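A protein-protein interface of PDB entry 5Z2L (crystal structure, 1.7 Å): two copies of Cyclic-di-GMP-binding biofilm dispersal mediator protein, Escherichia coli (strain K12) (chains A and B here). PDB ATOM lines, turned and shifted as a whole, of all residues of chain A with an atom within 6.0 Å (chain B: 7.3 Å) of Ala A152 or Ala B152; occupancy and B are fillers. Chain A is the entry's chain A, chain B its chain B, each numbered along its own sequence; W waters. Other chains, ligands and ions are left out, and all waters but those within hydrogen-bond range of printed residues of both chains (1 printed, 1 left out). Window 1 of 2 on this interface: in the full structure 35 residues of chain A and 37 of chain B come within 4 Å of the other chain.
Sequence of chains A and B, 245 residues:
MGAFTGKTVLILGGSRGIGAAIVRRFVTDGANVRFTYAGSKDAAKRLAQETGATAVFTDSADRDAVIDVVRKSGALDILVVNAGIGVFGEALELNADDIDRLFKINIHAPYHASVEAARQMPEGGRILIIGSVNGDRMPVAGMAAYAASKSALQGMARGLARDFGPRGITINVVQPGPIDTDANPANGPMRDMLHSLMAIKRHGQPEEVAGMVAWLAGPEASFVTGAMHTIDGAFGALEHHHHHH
O of Ala A148 sits at hydrogen-bond distance from OG of Ser A151, at 3.1 Å.
The side-chain hydroxyl (OG) of Ser B151 is in hydrogen-bond range of the backbone carbonyl oxygen (O) of Ala B148 (3.1 Å).
Among the printed residues, merely in contact across the chains: Ala A147 with Gly B155, Ala A148 with Ala B152, Ala A148 with Gly B155, Ala A148 with Met B156, Ala A152 with Ala B148, Ala A152 with Ala B152, Gly A155 with Ala B147, Gly A155 with Ala B148, Met A156 with Ala B144 and Met A156 with Ala B148.
Printed residues of chain B within 4 Å of Ala A152: Ala B148, Ser B151 and Ala B152.
Of the printed residues of chain A, Ala B152 touches Ala A148, Ser A151 and Ala A152.
Printed residues of chain B within 4 Å of Ala A147: Gly B155.
Of the printed residues of chain B, Gly A155 touches Ala B147 (3.8 Å), Ala B148 (3.8 Å) and Ser B151 (3.2 Å).
Of the printed residues of chain A, Ala B148 touches Ala A152 (3.3 Å), Gly A155 (3.8 Å) and Met A156 (3.6 Å).
Of the printed residues of chain A, Met B156 touches Ala A148 (3.6 Å).
Ala B157 touches none of the printed residues of chain A.
Among the printed residues, no Asp or Glu carboxylate lies within 4 Å of a Lys or Arg side-chain nitrogen of the other chain.
The backbone carbonyl oxygen of Ser B151 lies within hydrogen-bond range of the side-chain hydroxyl of Ser A151, at 2.7 Å.
The side-chain hydroxyl of Ser A151 sits at hydrogen-bond distance from the backbone carbonyl oxygen of Ala B152, at 3.1 Å.
The side-chain hydroxyl of Ser A151 sits at hydrogen-bond distance from the backbone NH of Gly B155 (3.2 Å).
The backbone carbonyl oxygen (O) of Ala A152 sits close to the side-chain hydroxyl (OG) of Ser B151, 3.3 Å away.
The backbone NH (N) of Gly A155 lies within hydrogen-bond range of the side-chain hydroxyl (OG) of Ser B151 (3.2 Å).
Water W1 lies within hydrogen-bond range of the side-chain amide oxygen (OE1) of Gln B154, the side-chain amide oxygen (OE1) of Gln A154 and the guanidinium group (NH1) of Arg B158.
Ala A147 touches Gly B155, and with the chains exchanged Gly A155 touches Ala B147.
Ala A148 touches Met B156, and with the chains exchanged Met A156 touches Ala B148.
Ser A151 touches Ala B152, and with the chains exchanged Ala A152 touches Ser B151.
Ala A152 touches its own counterpart, Ala B152.
Of the 15 pairs that touch across the chains among the printed residues, 14 have their exchanged pair printed and touching as well.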
ATOM      1  N   ILE A 107      -0.406   5.953  15.007  1.00  0.00           N
ATOM      2  CA  ILE A 107       0.922   5.765  15.598  1.00  0.00           C
ATOM      3  C   ILE A 107       1.357   7.004  16.384  1.00  0.00           C
ATOM      4  O   ILE A 107       1.663   6.921  17.572  1.00  0.00           O
ATOM      5  CB  ILE A 107       1.971   5.401  14.524  1.00  0.00           C
ATOM      6  CG1 ILE A 107       1.522   4.217  13.671  1.00  0.00           C
ATOM      7  CG2 ILE A 107       3.328   5.086  15.189  1.00  0.00           C
ATOM      8  CD1 ILE A 107       2.502   3.899  12.562  1.00  0.00           C
ATOM      9  N   ALA A 147      -2.285  -2.461   9.557  1.00  0.00           N
ATOM     10  CA  ALA A 147      -1.635  -3.485  10.374  1.00  0.00           C
ATOM     11  C   ALA A 147      -0.313  -2.987  10.937  1.00  0.00           C
ATOM     12  O   ALA A 147       0.001  -3.234  12.106  1.00  0.00           O
ATOM     13  CB  ALA A 147      -1.410  -4.762   9.559  1.00  0.00           C
ATOM     14  N   ALA A 148       0.489  -2.314  10.112  1.00  0.00           N
ATOM     15  CA  ALA A 148       1.725  -1.726  10.612  1.00  0.00           C
ATOM     16  C   ALA A 148       1.456  -0.771  11.764  1.00  0.00           C
ATOM     17  O   ALA A 148       2.195  -0.759  12.758  1.00  0.00           O
ATOM     18  CB  ALA A 148       2.467  -1.001   9.492  1.00  0.00           C
ATOM     19  N   SER A 149       0.419   0.060  11.640  1.00  0.00           N
ATOM     20  CA  SER A 149       0.160   1.036  12.690  1.00  0.00           C
ATOM     21  C   SER A 149      -0.231   0.346  13.986  1.00  0.00           C
ATOM     22  O   SER A 149       0.158   0.798  15.070  1.00  0.00           O
ATOM     23  CB  SER A 149      -0.919   2.041  12.239  1.00  0.00           C
ATOM     24  OG  SER A 149      -2.211   1.456  12.261  1.00  0.00           O
ATOM     25  N   LYS A 150      -0.915  -0.793  13.898  1.00  0.00           N
ATOM     26  CA  LYS A 150      -1.301  -1.498  15.118  1.00  0.00           C
ATOM     27  C   LYS A 150      -0.164  -2.347  15.696  1.00  0.00           C
ATOM     28  O   LYS A 150      -0.093  -2.535  16.916  1.00  0.00           O
ATOM     29  CB  LYS A 150      -2.543  -2.345  14.838  1.00  0.00           C
ATOM     30  CG  LYS A 150      -3.776  -1.484  14.456  1.00  0.00           C
ATOM     31  CD  LYS A 150      -4.163  -0.474  15.557  1.00  0.00           C
ATOM     32  CE  LYS A 150      -5.533   0.208  15.279  1.00  0.00           C
ATOM     33  NZ  LYS A 150      -5.964   1.143  16.380  1.00  0.00           N
ATOM     34  N   SER A 151       0.744  -2.853  14.861  1.00  0.00           N
ATOM     35  CA  SER A 151       1.922  -3.524  15.414  1.00  0.00           C
ATOM     36  C   SER A 151       2.871  -2.524  16.070  1.00  0.00           C
ATOM     37  O   SER A 151       3.554  -2.876  17.043  1.00  0.00           O
ATOM     38  CB  SER A 151       2.648  -4.345  14.340  1.00  0.00           C
ATOM     39  OG  SER A 151       3.287  -3.568  13.351  1.00  0.00           O
ATOM     40  N   ALA A 152       2.895  -1.270  15.579  1.00  0.00           N
ATOM     41  CA  ALA A 152       3.736  -0.233  16.187  1.00  0.00           C
ATOM     42  C   ALA A 152       3.442  -0.064  17.671  1.00  0.00           C
ATOM     43  O   ALA A 152       4.337   0.303  18.460  1.00  0.00           O
ATOM     44  CB  ALA A 152       3.528   1.106  15.462  1.00  0.00           C
ATOM     45  N   LEU A 153       2.181  -0.271  18.060  1.00  0.00           N
ATOM     46  CA  LEU A 153       1.779  -0.041  19.442  1.00  0.00           C
ATOM     47  C   LEU A 153       2.401  -1.051  20.386  1.00  0.00           C
ATOM     48  O   LEU A 153       2.531  -0.776  21.584  1.00  0.00           O
ATOM     49  CB  LEU A 153       0.254  -0.083  19.568  1.00  0.00           C
ATOM     50  CG  LEU A 153      -0.475   0.902  18.665  1.00  0.00           C
ATOM     51  CD1 LEU A 153      -1.967   0.718  18.804  1.00  0.00           C
ATOM     52  CD2 LEU A 153      -0.065   2.340  19.019  1.00  0.00           C
ATOM     53  N   GLN A 154       2.826  -2.202  19.869  1.00  0.00           N
ATOM     54  CA  GLN A 154       3.381  -3.236  20.729  1.00  0.00           C
ATOM     55  C   GLN A 154       4.746  -2.812  21.260  1.00  0.00           C
ATOM     56  O   GLN A 154       4.976  -2.777  22.476  1.00  0.00           O
ATOM     57  CB  GLN A 154       3.452  -4.550  19.941  1.00  0.00           C
ATOM     58  CG  GLN A 154       2.086  -4.943  19.383  1.00  0.00           C
ATOM     59  CD  GLN A 154       2.123  -6.158  18.466  1.00  0.00           C
ATOM     60  OE1 GLN A 154       3.163  -6.491  17.893  1.00  0.00           O
ATOM     61  NE2 GLN A 154       0.976  -6.809  18.308  1.00  0.00           N
ATOM     62  N   GLY A 155       5.667  -2.488  20.356  1.00  0.00           N
ATOM     63  CA  GLY A 155       6.951  -1.979  20.788  1.00  0.00           C
ATOM     64  C   GLY A 155       6.800  -0.693  21.569  1.00  0.00           C
ATOM     65  O   GLY A 155       7.518  -0.458  22.556  1.00  0.00           O
ATOM     66  N   MET A 156       5.842   0.145  21.149  1.00  0.00           N
ATOM     67  CA  MET A 156       5.589   1.396  21.857  1.00  0.00           C
ATOM     68  C   MET A 156       5.239   1.153  23.325  1.00  0.00           C
ATOM     69  O   MET A 156       5.782   1.806  24.224  1.00  0.00           O
ATOM     70  CB  MET A 156       4.458   2.154  21.172  1.00  0.00           C
ATOM     71  CG  MET A 156       4.314   3.550  21.723  1.00  0.00           C
ATOM     72  SD  MET A 156       2.922   4.422  20.982  1.00  0.00           S
ATOM     73  CE  MET A 156       3.452   4.467  19.271  1.00  0.00           C
ATOM     74  N   ALA A 157       4.292   0.251  23.579  1.00  0.00           N
ATOM     75  CA  ALA A 157       3.839  -0.034  24.934  1.00  0.00           C
ATOM     76  C   ALA A 157       4.916  -0.724  25.760  1.00  0.00           C
ATOM     77  O   ALA A 157       5.084  -0.410  26.944  1.00  0.00           O
ATOM     78  CB  ALA A 157       2.583  -0.902  24.889  1.00  0.00           C
ATOM     79  N   PHE B 103       9.949   8.479  13.235  1.00  0.00           N
ATOM     80  CA  PHE B 103       8.821   7.770  12.629  1.00  0.00           C
ATOM     81  C   PHE B 103       8.848   7.885  11.109  1.00  0.00           C
ATOM     82  O   PHE B 103       8.547   6.916  10.395  1.00  0.00           O
ATOM     83  CB  PHE B 103       7.493   8.328  13.149  1.00  0.00           C
ATOM     84  CG  PHE B 103       7.195   7.986  14.580  1.00  0.00           C
ATOM     85  CD1 PHE B 103       7.687   6.820  15.161  1.00  0.00           C
ATOM     86  CD2 PHE B 103       6.404   8.835  15.345  1.00  0.00           C
ATOM     87  CE1 PHE B 103       7.393   6.506  16.492  1.00  0.00           C
ATOM     88  CE2 PHE B 103       6.106   8.527  16.663  1.00  0.00           C
ATOM     89  CZ  PHE B 103       6.596   7.370  17.240  1.00  0.00           C
ATOM     90  N   ASN B 106      11.897   5.625   9.866  1.00  0.00           N
ATOM     91  CA  ASN B 106      11.872   4.213  10.248  1.00  0.00           C
ATOM     92  C   ASN B 106      10.568   3.519   9.875  1.00  0.00           C
ATOM     93  O   ASN B 106      10.558   2.291   9.724  1.00  0.00           O
ATOM     94  CB  ASN B 106      12.087   4.064  11.763  1.00  0.00           C
ATOM     95  CG  ASN B 106      13.510   4.400  12.202  1.00  0.00           C
ATOM     96  OD1 ASN B 106      14.295   4.996  11.455  1.00  0.00           O
ATOM     97  ND2 ASN B 106      13.849   4.003  13.434  1.00  0.00           N
ATOM     98  N   ILE B 107       9.463   4.264   9.751  1.00  0.00           N
ATOM     99  CA  ILE B 107       8.148   3.685   9.454  1.00  0.00           C
ATOM    100  C   ILE B 107       7.651   4.103   8.076  1.00  0.00           C
ATOM    101  O   ILE B 107       7.341   3.257   7.233  1.00  0.00           O
ATOM    102  CB  ILE B 107       7.112   4.044  10.542  1.00  0.00           C
ATOM    103  CG1 ILE B 107       7.604   3.673  11.935  1.00  0.00           C
ATOM    104  CG2 ILE B 107       5.784   3.360  10.241  1.00  0.00           C
ATOM    105  CD1 ILE B 107       6.608   4.065  13.025  1.00  0.00           C
ATOM    106  N   GLY B 135      12.032  -4.860  17.701  1.00  0.00           N
ATOM    107  CA  GLY B 135      10.629  -4.982  17.351  1.00  0.00           C
ATOM    108  C   GLY B 135       9.907  -6.075  18.116  1.00  0.00           C
ATOM    109  O   GLY B 135       8.678  -6.022  18.238  1.00  0.00           O
ATOM    110  N   ALA B 144      11.571   3.841  23.393  1.00  0.00           N
ATOM    111  CA  ALA B 144      10.190   3.433  23.161  1.00  0.00           C
ATOM    112  C   ALA B 144       9.755   3.732  21.725  1.00  0.00           C
ATOM    113  O   ALA B 144       9.176   2.872  21.049  1.00  0.00           O
ATOM    114  CB  ALA B 144       9.275   4.122  24.174  1.00  0.00           C
ATOM    115  N   ALA B 145      10.021   4.950  21.239  1.00  0.00           N
ATOM    116  CA  ALA B 145       9.642   5.285  19.867  1.00  0.00           C
ATOM    117  C   ALA B 145      10.414   4.444  18.850  1.00  0.00           C
ATOM    118  O   ALA B 145       9.841   3.977  17.862  1.00  0.00           O
ATOM    119  CB  ALA B 145       9.859   6.777  19.606  1.00  0.00           C
ATOM    120  N   TYR B 146      11.711   4.225  19.080  1.00  0.00           N
ATOM    121  CA  TYR B 146      12.484   3.367  18.185  1.00  0.00           C
ATOM    122  C   TYR B 146      11.887   1.964  18.124  1.00  0.00           C
ATOM    123  O   TYR B 146      11.693   1.389  17.037  1.00  0.00           O
ATOM    124  CB  TYR B 146      13.942   3.318  18.652  1.00  0.00           C
ATOM    125  CG  TYR B 146      14.814   2.354  17.865  1.00  0.00           C
ATOM    126  CD1 TYR B 146      15.312   2.709  16.616  1.00  0.00           C
ATOM    127  CD2 TYR B 146      15.152   1.098  18.371  1.00  0.00           C
ATOM    128  CE1 TYR B 146      16.118   1.848  15.890  1.00  0.00           C
ATOM    129  CE2 TYR B 146      15.964   0.228  17.650  1.00  0.00           C
ATOM    130  CZ  TYR B 146      16.441   0.615  16.410  1.00  0.00           C
ATOM    131  OH  TYR B 146      17.243  -0.222  15.655  1.00  0.00           O
ATOM    132  N   ALA B 147      11.600   1.386  19.296  1.00  0.00           N
ATOM    133  CA  ALA B 147      11.025   0.044  19.339  1.00  0.00           C
ATOM    134  C   ALA B 147       9.681   0.008  18.625  1.00  0.00           C
ATOM    135  O   ALA B 147       9.371  -0.945  17.901  1.00  0.00           O
ATOM    136  CB  ALA B 147      10.889  -0.414  20.787  1.00  0.00           C
ATOM    137  N   ALA B 148       8.855   1.038  18.836  1.00  0.00           N
ATOM    138  CA  ALA B 148       7.600   1.130  18.107  1.00  0.00           C
ATOM    139  C   ALA B 148       7.836   1.114  16.603  1.00  0.00           C
ATOM    140  O   ALA B 148       7.097   0.457  15.859  1.00  0.00           O
ATOM    141  CB  ALA B 148       6.834   2.391  18.525  1.00  0.00           C
ATOM    142  N   SER B 149       8.848   1.850  16.133  1.00  0.00           N
ATOM    143  CA  SER B 149       9.084   1.912  14.696  1.00  0.00           C
ATOM    144  C   SER B 149       9.510   0.561  14.155  1.00  0.00           C
ATOM    145  O   SER B 149       9.197   0.229  13.006  1.00  0.00           O
ATOM    146  CB  SER B 149      10.133   2.977  14.360  1.00  0.00           C
ATOM    147  OG  SER B 149      11.443   2.557  14.717  1.00  0.00           O
ATOM    148  N   LYS B 150      10.211  -0.235  14.965  1.00  0.00           N
ATOM    149  CA  LYS B 150      10.659  -1.532  14.471  1.00  0.00           C
ATOM    150  C   LYS B 150       9.561  -2.588  14.556  1.00  0.00           C
ATOM    151  O   LYS B 150       9.512  -3.479  13.703  1.00  0.00           O
ATOM    152  CB  LYS B 150      11.903  -1.967  15.233  1.00  0.00           C
ATOM    153  CG  LYS B 150      13.069  -1.002  15.014  1.00  0.00           C
ATOM    154  CD  LYS B 150      13.397  -0.894  13.528  1.00  0.00           C
ATOM    155  CE  LYS B 150      14.722  -0.181  13.289  1.00  0.00           C
ATOM    156  NZ  LYS B 150      15.095  -0.126  11.833  1.00  0.00           N
ATOM    157  N   SER B 151       8.669  -2.497  15.550  1.00  0.00           N
ATOM    158  CA  SER B 151       7.515  -3.394  15.577  1.00  0.00           C
ATOM    159  C   SER B 151       6.531  -3.064  14.458  1.00  0.00           C
ATOM    160  O   SER B 151       5.848  -3.965  13.953  1.00  0.00           O
ATOM    161  CB  SER B 151       6.803  -3.352  16.941  1.00  0.00           C
ATOM    162  OG  SER B 151       6.152  -2.128  17.182  1.00  0.00           O
ATOM    163  N   ALA B 152       6.458  -1.789  14.054  1.00  0.00           N
ATOM    164  CA  ALA B 152       5.585  -1.389  12.950  1.00  0.00           C
ATOM    165  C   ALA B 152       5.873  -2.194  11.689  1.00  0.00           C
ATOM    166  O   ALA B 152       4.954  -2.527  10.915  1.00  0.00           O
ATOM    167  CB  ALA B 152       5.764   0.105  12.675  1.00  0.00           C
ATOM    168  N   LEU B 153       7.149  -2.526  11.479  1.00  0.00           N
ATOM    169  CA  LEU B 153       7.575  -3.222  10.276  1.00  0.00           C
ATOM    170  C   LEU B 153       7.026  -4.632  10.206  1.00  0.00           C
ATOM    171  O   LEU B 153       6.955  -5.196   9.108  1.00  0.00           O
ATOM    172  CB  LEU B 153       9.099  -3.272  10.205  1.00  0.00           C
ATOM    173  CG  LEU B 153       9.815  -1.919  10.238  1.00  0.00           C
ATOM    174  CD1 LEU B 153      11.320  -2.181  10.254  1.00  0.00           C
ATOM    175  CD2 LEU B 153       9.439  -1.066   9.038  1.00  0.00           C
ATOM    176  N   GLN B 154       6.639  -5.210  11.345  1.00  0.00           N
ATOM    177  CA  GLN B 154       6.156  -6.585  11.362  1.00  0.00           C
ATOM    178  C   GLN B 154       4.786  -6.685  10.697  1.00  0.00           C
ATOM    179  O   GLN B 154       4.594  -7.463   9.749  1.00  0.00           O
ATOM    180  CB  GLN B 154       6.143  -7.092  12.807  1.00  0.00           C
ATOM    181  CG  GLN B 154       7.539  -6.992  13.451  1.00  0.00           C
ATOM    182  CD  GLN B 154       7.557  -7.329  14.938  1.00  0.00           C
ATOM    183  OE1 GLN B 154       6.543  -7.228  15.626  1.00  0.00           O
ATOM    184  NE2 GLN B 154       8.712  -7.748  15.435  1.00  0.00           N
ATOM    185  N   GLY B 155       3.818  -5.888  11.181  1.00  0.00           N
ATOM    186  CA  GLY B 155       2.523  -5.829  10.520  1.00  0.00           C
ATOM    187  C   GLY B 155       2.656  -5.344   9.093  1.00  0.00           C
ATOM    188  O   GLY B 155       1.949  -5.818   8.195  1.00  0.00           O
ATOM    189  N   MET B 156       3.582  -4.403   8.863  1.00  0.00           N
ATOM    190  CA  MET B 156       3.807  -3.903   7.515  1.00  0.00           C
ATOM    191  C   MET B 156       4.183  -5.023   6.553  1.00  0.00           C
ATOM    192  O   MET B 156       3.604  -5.144   5.469  1.00  0.00           O
ATOM    193  CB  MET B 156       4.904  -2.844   7.531  1.00  0.00           C
ATOM    194  CG  MET B 156       5.017  -2.099   6.219  1.00  0.00           C
ATOM    195  SD  MET B 156       6.344  -0.873   6.196  1.00  0.00           S
ATOM    196  CE  MET B 156       5.789   0.261   7.481  1.00  0.00           C
ATOM    197  N   ALA B 157       5.175  -5.830   6.924  1.00  0.00           N
ATOM    198  CA  ALA B 157       5.666  -6.898   6.048  1.00  0.00           C
ATOM    199  C   ALA B 157       4.643  -8.014   5.891  1.00  0.00           C
ATOM    200  O   ALA B 157       4.481  -8.561   4.792  1.00  0.00           O
ATOM    201  CB  ALA B 157       6.978  -7.467   6.595  1.00  0.00           C
ATOM    202  N   ARG B 158       3.949  -8.377   6.969  1.00  0.00           N
ATOM    203  CA  ARG B 158       2.912  -9.392   6.824  1.00  0.00           C
ATOM    204  C   ARG B 158       1.838  -8.926   5.850  1.00  0.00           C
ATOM    205  O   ARG B 158       1.405  -9.697   4.985  1.00  0.00           O
ATOM    206  CB  ARG B 158       2.282  -9.719   8.174  1.00  0.00           C
ATOM    207  CG  ARG B 158       3.245 -10.301   9.195  1.00  0.00           C
ATOM    208  CD  ARG B 158       2.522 -10.447  10.535  1.00  0.00           C
ATOM    209  NE  ARG B 158       3.428 -10.735  11.643  1.00  0.00           N
ATOM    210  CZ  ARG B 158       3.475 -10.033  12.776  1.00  0.00           C
ATOM    211  NH1 ARG B 158       2.657  -9.004  12.964  1.00  0.00           N
ATOM    212  NH2 ARG B 158       4.339 -10.367  13.729  1.00  0.00           N
ATOM    213  N   VAL B 173      11.549  -9.009   6.671  1.00  0.00           N
ATOM    214  CA  VAL B 173      12.225  -8.109   7.602  1.00  0.00           C
ATOM    215  C   VAL B 173      13.355  -8.893   8.252  1.00  0.00           C
ATOM    216  O   VAL B 173      13.131  -9.992   8.772  1.00  0.00           O
ATOM    217  CB  VAL B 173      11.254  -7.571   8.669  1.00  0.00           C
ATOM    218  CG1 VAL B 173      11.987  -6.706   9.688  1.00  0.00           C
ATOM    219  CG2 VAL B 173      10.096  -6.819   8.009  1.00  0.00           C
HETATM  220  O   HOH W   1       3.855  -7.830  15.446  1.00  0.00           O
